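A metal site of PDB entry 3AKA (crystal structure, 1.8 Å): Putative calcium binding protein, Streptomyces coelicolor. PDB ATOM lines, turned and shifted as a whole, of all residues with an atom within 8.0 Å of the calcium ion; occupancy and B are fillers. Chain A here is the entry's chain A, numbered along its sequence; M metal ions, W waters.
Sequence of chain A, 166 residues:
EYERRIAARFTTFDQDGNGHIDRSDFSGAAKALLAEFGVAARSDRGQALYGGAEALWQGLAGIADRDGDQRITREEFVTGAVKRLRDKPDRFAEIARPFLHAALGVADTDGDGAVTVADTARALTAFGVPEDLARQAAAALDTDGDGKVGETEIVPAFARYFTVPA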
ATOM      1  N   HIS A  20       3.873   7.216  -6.291  1.00  0.00           N
ATOM      2  CA  HIS A  20       4.675   7.226  -5.067  1.00  0.00           C
ATOM      3  C   HIS A  20       3.770   7.509  -3.873  1.00  0.00           C
ATOM      4  O   HIS A  20       2.767   8.200  -3.991  1.00  0.00           O
ATOM      5  CB  HIS A  20       5.838   8.259  -5.122  1.00  0.00           C
ATOM      6  CG  HIS A  20       5.397   9.650  -5.442  1.00  0.00           C
ATOM      7  ND1 HIS A  20       5.058  10.567  -4.477  1.00  0.00           N
ATOM      8  CD2 HIS A  20       5.261  10.289  -6.620  1.00  0.00           C
ATOM      9  CE1 HIS A  20       4.691  11.699  -5.044  1.00  0.00           C
ATOM     10  NE2 HIS A  20       4.844  11.573  -6.352  1.00  0.00           N
ATOM     11  N   ILE A  21       4.152   6.984  -2.723  1.00  0.00           N
ATOM     12  CA  ILE A  21       3.389   7.232  -1.517  1.00  0.00           C
ATOM     13  C   ILE A  21       4.007   8.460  -0.828  1.00  0.00           C
ATOM     14  O   ILE A  21       5.228   8.469  -0.612  1.00  0.00           O
ATOM     15  CB  ILE A  21       3.430   6.024  -0.605  1.00  0.00           C
ATOM     16  CG1 ILE A  21       2.954   4.765  -1.364  1.00  0.00           C
ATOM     17  CG2 ILE A  21       2.525   6.257   0.589  1.00  0.00           C
ATOM     18  CD1 ILE A  21       3.295   3.461  -0.571  1.00  0.00           C
ATOM     19  N   TRP A  57       1.915   6.973   8.172  1.00  0.00           N
ATOM     20  CA  TRP A  57       2.848   7.445   7.129  1.00  0.00           C
ATOM     21  C   TRP A  57       4.311   7.390   7.655  1.00  0.00           C
ATOM     22  O   TRP A  57       5.209   6.921   6.970  1.00  0.00           O
ATOM     23  CB  TRP A  57       2.494   8.882   6.698  1.00  0.00           C
ATOM     24  CG  TRP A  57       3.711   9.632   6.118  1.00  0.00           C
ATOM     25  CD1 TRP A  57       4.358  10.686   6.684  1.00  0.00           C
ATOM     26  CD2 TRP A  57       4.403   9.321   4.910  1.00  0.00           C
ATOM     27  NE1 TRP A  57       5.434  11.059   5.887  1.00  0.00           N
ATOM     28  CE2 TRP A  57       5.490  10.237   4.799  1.00  0.00           C
ATOM     29  CE3 TRP A  57       4.239   8.346   3.920  1.00  0.00           C
ATOM     30  CZ2 TRP A  57       6.395  10.205   3.715  1.00  0.00           C
ATOM     31  CZ3 TRP A  57       5.130   8.318   2.838  1.00  0.00           C
ATOM     32  CH2 TRP A  57       6.188   9.254   2.740  1.00  0.00           C
ATOM     33  N   ALA A  61       7.156   5.118   6.051  1.00  0.00           N
ATOM     34  CA  ALA A  61       8.343   5.816   5.544  1.00  0.00           C
ATOM     35  C   ALA A  61       9.589   5.273   6.217  1.00  0.00           C
ATOM     36  O   ALA A  61      10.588   5.038   5.542  1.00  0.00           O
ATOM     37  CB  ALA A  61       8.239   7.321   5.776  1.00  0.00           C
ATOM     38  N   ALA A  64      10.238   1.958   4.421  1.00  0.00           N
ATOM     39  CA  ALA A  64      10.338   1.857   2.966  1.00  0.00           C
ATOM     40  C   ALA A  64      10.997   3.041   2.239  1.00  0.00           C
ATOM     41  O   ALA A  64      11.405   2.881   1.080  1.00  0.00           O
ATOM     42  CB  ALA A  64       8.959   1.590   2.361  1.00  0.00           C
ATOM     43  N   ASP A  65      11.069   4.221   2.865  1.00  0.00           N
ATOM     44  CA  ASP A  65      11.673   5.363   2.180  1.00  0.00           C
ATOM     45  C   ASP A  65      13.209   5.282   2.304  1.00  0.00           C
ATOM     46  O   ASP A  65      13.818   5.956   3.145  1.00  0.00           O
ATOM     47  CB  ASP A  65      11.153   6.699   2.740  1.00  0.00           C
ATOM     48  CG  ASP A  65      11.710   7.921   2.007  1.00  0.00           C
ATOM     49  OD1 ASP A  65      12.093   7.805   0.846  1.00  0.00           O
ATOM     50  OD2 ASP A  65      11.740   9.018   2.619  1.00  0.00           O
ATOM     51  N   ARG A  66      13.831   4.477   1.452  1.00  0.00           N
ATOM     52  CA  ARG A  66      15.266   4.186   1.566  1.00  0.00           C
ATOM     53  C   ARG A  66      16.197   5.369   1.271  1.00  0.00           C
ATOM     54  O   ARG A  66      17.315   5.406   1.780  1.00  0.00           O
ATOM     55  CB  ARG A  66      15.631   3.013   0.650  1.00  0.00           C
ATOM     56  CG  ARG A  66      14.748   1.754   0.813  1.00  0.00           C
ATOM     57  CD  ARG A  66      14.772   1.183   2.221  1.00  0.00           C
ATOM     58  NE  ARG A  66      16.078   0.596   2.601  1.00  0.00           N
ATOM     59  CZ  ARG A  66      16.369   0.165   3.830  1.00  0.00           C
ATOM     60  NH1 ARG A  66      15.453   0.235   4.805  1.00  0.00           N
ATOM     61  NH2 ARG A  66      17.564  -0.357   4.088  1.00  0.00           N
ATOM     62  N   ASP A  67      15.757   6.319   0.433  1.00  0.00           N
ATOM     63  CA  ASP A  67      16.622   7.467   0.085  1.00  0.00           C
ATOM     64  C   ASP A  67      16.274   8.753   0.856  1.00  0.00           C
ATOM     65  O   ASP A  67      16.928   9.799   0.682  1.00  0.00           O
ATOM     66  CB  ASP A  67      16.716   7.696  -1.428  1.00  0.00           C
ATOM     67  CG  ASP A  67      15.394   8.083  -2.065  1.00  0.00           C
ATOM     68  OD1 ASP A  67      14.420   8.372  -1.344  1.00  0.00           O
ATOM     69  OD2 ASP A  67      15.329   8.044  -3.316  1.00  0.00           O
ATOM     70  N   GLY A  68      15.241   8.672   1.702  1.00  0.00           N
ATOM     71  CA  GLY A  68      14.893   9.755   2.610  1.00  0.00           C
ATOM     72  C   GLY A  68      14.271  10.996   1.997  1.00  0.00           C
ATOM     73  O   GLY A  68      14.274  12.032   2.638  1.00  0.00           O
ATOM     74  N   ASP A  69      13.768  10.917   0.759  1.00  0.00           N
ATOM     75  CA  ASP A  69      13.113  12.066   0.121  1.00  0.00           C
ATOM     76  C   ASP A  69      11.637  12.218   0.503  1.00  0.00           C
ATOM     77  O   ASP A  69      10.940  13.108  -0.012  1.00  0.00           O
ATOM     78  CB  ASP A  69      13.301  12.060  -1.401  1.00  0.00           C
ATOM     79  CG  ASP A  69      12.505  10.943  -2.093  1.00  0.00           C
ATOM     80  OD1 ASP A  69      11.934  10.084  -1.362  1.00  0.00           O
ATOM     81  OD2 ASP A  69      12.420  10.965  -3.344  1.00  0.00           O
ATOM     82  N   GLN A  70      11.158  11.368   1.409  1.00  0.00           N
ATOM     83  CA  GLN A  70       9.781  11.462   1.879  1.00  0.00           C
ATOM     84  C   GLN A  70       8.711  11.237   0.789  1.00  0.00           C
ATOM     85  O   GLN A  70       7.602  11.798   0.845  1.00  0.00           O
ATOM     86  CB  GLN A  70       9.596  12.759   2.691  1.00  0.00           C
ATOM     87  CG  GLN A  70      10.430  12.706   3.971  1.00  0.00           C
ATOM     88  CD  GLN A  70      10.454  14.030   4.706  1.00  0.00           C
ATOM     89  OE1 GLN A  70       9.959  15.054   4.215  1.00  0.00           O
ATOM     90  NE2 GLN A  70      11.055  14.016   5.897  1.00  0.00           N
ATOM     91  N   ARG A  71       9.076  10.430  -0.205  1.00  0.00           N
ATOM     92  CA  ARG A  71       8.123   9.817  -1.130  1.00  0.00           C
ATOM     93  C   ARG A  71       8.543   8.341  -1.184  1.00  0.00           C
ATOM     94  O   ARG A  71       9.729   8.035  -1.232  1.00  0.00           O
ATOM     95  CB  ARG A  71       8.237  10.424  -2.535  1.00  0.00           C
ATOM     96  CG  ARG A  71       8.002  11.909  -2.611  1.00  0.00           C
ATOM     97  CD  ARG A  71       8.035  12.432  -4.073  1.00  0.00           C
ATOM     98  NE  ARG A  71       9.416  12.567  -4.484  1.00  0.00           N
ATOM     99  CZ  ARG A  71      10.053  13.732  -4.582  1.00  0.00           C
ATOM    100  NH1 ARG A  71       9.414  14.877  -4.353  1.00  0.00           N
ATOM    101  NH2 ARG A  71      11.335  13.749  -4.944  1.00  0.00           N
ATOM    102  N   ILE A  72       7.601   7.427  -1.173  1.00  0.00           N
ATOM    103  CA  ILE A  72       7.959   6.009  -1.317  1.00  0.00           C
ATOM    104  C   ILE A  72       7.563   5.598  -2.731  1.00  0.00           C
ATOM    105  O   ILE A  72       6.372   5.584  -3.049  1.00  0.00           O
ATOM    106  CB  ILE A  72       7.170   5.172  -0.295  1.00  0.00           C
ATOM    107  CG1 ILE A  72       7.381   5.706   1.136  1.00  0.00           C
ATOM    108  CG2 ILE A  72       7.492   3.647  -0.465  1.00  0.00           C
ATOM    109  CD1 ILE A  72       6.609   4.891   2.246  1.00  0.00           C
ATOM    110  N   THR A  73       8.536   5.266  -3.572  1.00  0.00           N
ATOM    111  CA  THR A  73       8.280   4.874  -4.952  1.00  0.00           C
ATOM    112  C   THR A  73       7.748   3.422  -4.994  1.00  0.00           C
ATOM    113  O   THR A  73       7.916   2.662  -4.036  1.00  0.00           O
ATOM    114  CB  THR A  73       9.560   4.955  -5.840  1.00  0.00           C
ATOM    115  OG1 THR A  73      10.542   4.037  -5.330  1.00  0.00           O
ATOM    116  CG2 THR A  73      10.144   6.382  -5.839  1.00  0.00           C
ATOM    117  N   GLU A  76      10.799   1.279  -4.303  1.00  0.00           N
ATOM    118  CA  GLU A  76      11.115   1.235  -2.890  1.00  0.00           C
ATOM    119  C   GLU A  76      10.147   0.357  -2.124  1.00  0.00           C
ATOM    120  O   GLU A  76      10.552  -0.376  -1.218  1.00  0.00           O
ATOM    121  CB  GLU A  76      11.045   2.645  -2.293  1.00  0.00           C
ATOM    122  CG  GLU A  76      12.310   3.427  -2.482  1.00  0.00           C
ATOM    123  CD  GLU A  76      12.185   4.867  -2.010  1.00  0.00           C
ATOM    124  OE1 GLU A  76      11.133   5.530  -2.249  1.00  0.00           O
ATOM    125  OE2 GLU A  76      13.164   5.339  -1.412  1.00  0.00           O
ATOM    126  N   PHE A  77       8.869   0.459  -2.481  1.00  0.00           N
ATOM    127  CA  PHE A  77       7.859  -0.406  -1.895  1.00  0.00           C
ATOM    128  C   PHE A  77       8.141  -1.881  -2.252  1.00  0.00           C
ATOM    129  O   PHE A  77       8.146  -2.719  -1.350  1.00  0.00           O
ATOM    130  CB  PHE A  77       6.451  -0.018  -2.338  1.00  0.00           C
ATOM    131  CG  PHE A  77       5.389  -0.647  -1.510  1.00  0.00           C
ATOM    132  CD1 PHE A  77       5.116  -0.164  -0.233  1.00  0.00           C
ATOM    133  CD2 PHE A  77       4.699  -1.777  -1.963  1.00  0.00           C
ATOM    134  CE1 PHE A  77       4.157  -0.771   0.593  1.00  0.00           C
ATOM    135  CE2 PHE A  77       3.743  -2.397  -1.144  1.00  0.00           C
ATOM    136  CZ  PHE A  77       3.477  -1.885   0.128  1.00  0.00           C
HETATM  137 CA    CA M   1      12.105   7.611  -1.424  1.00  0.00          CA
HETATM  138  O   HOH W   1      12.591   7.970  -3.648  1.00  0.00           O
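The side-chain carboxylate of Glu 76 sits close to the backbone NH of Arg 66, at 3.1 Å.
N of Gly 68 lies close to OD1 of Asp 65, 3.4 Å away.
OD2 of Asp 65 is in hydrogen-bond range of N of Gln 70 (2.7 Å).
N of Glu 76 sits at hydrogen-bond distance from OG1 of Thr 73 (3.0 Å).
Five residues have an atom within 4 Å of the calcium ion: Asp 65, Asp 67, Asp 69, Arg 71 and Glu 76.
The nearest printed residue that does not touch the calcium ion is Ile 72 (4.4 Å).
The calcium ion is bound by OD1 of Asp 65, water W1, O of Arg 71, OD1 of Asp 67, OE1 of Glu 76, OD1 of Asp 69 and OE2 of Glu 76.
Water W1 lies within hydrogen-bond range of the side-chain carboxylate of Asp 67 (2.8 Å) and the side-chain carboxylate of Asp 69 (3.0 Å).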
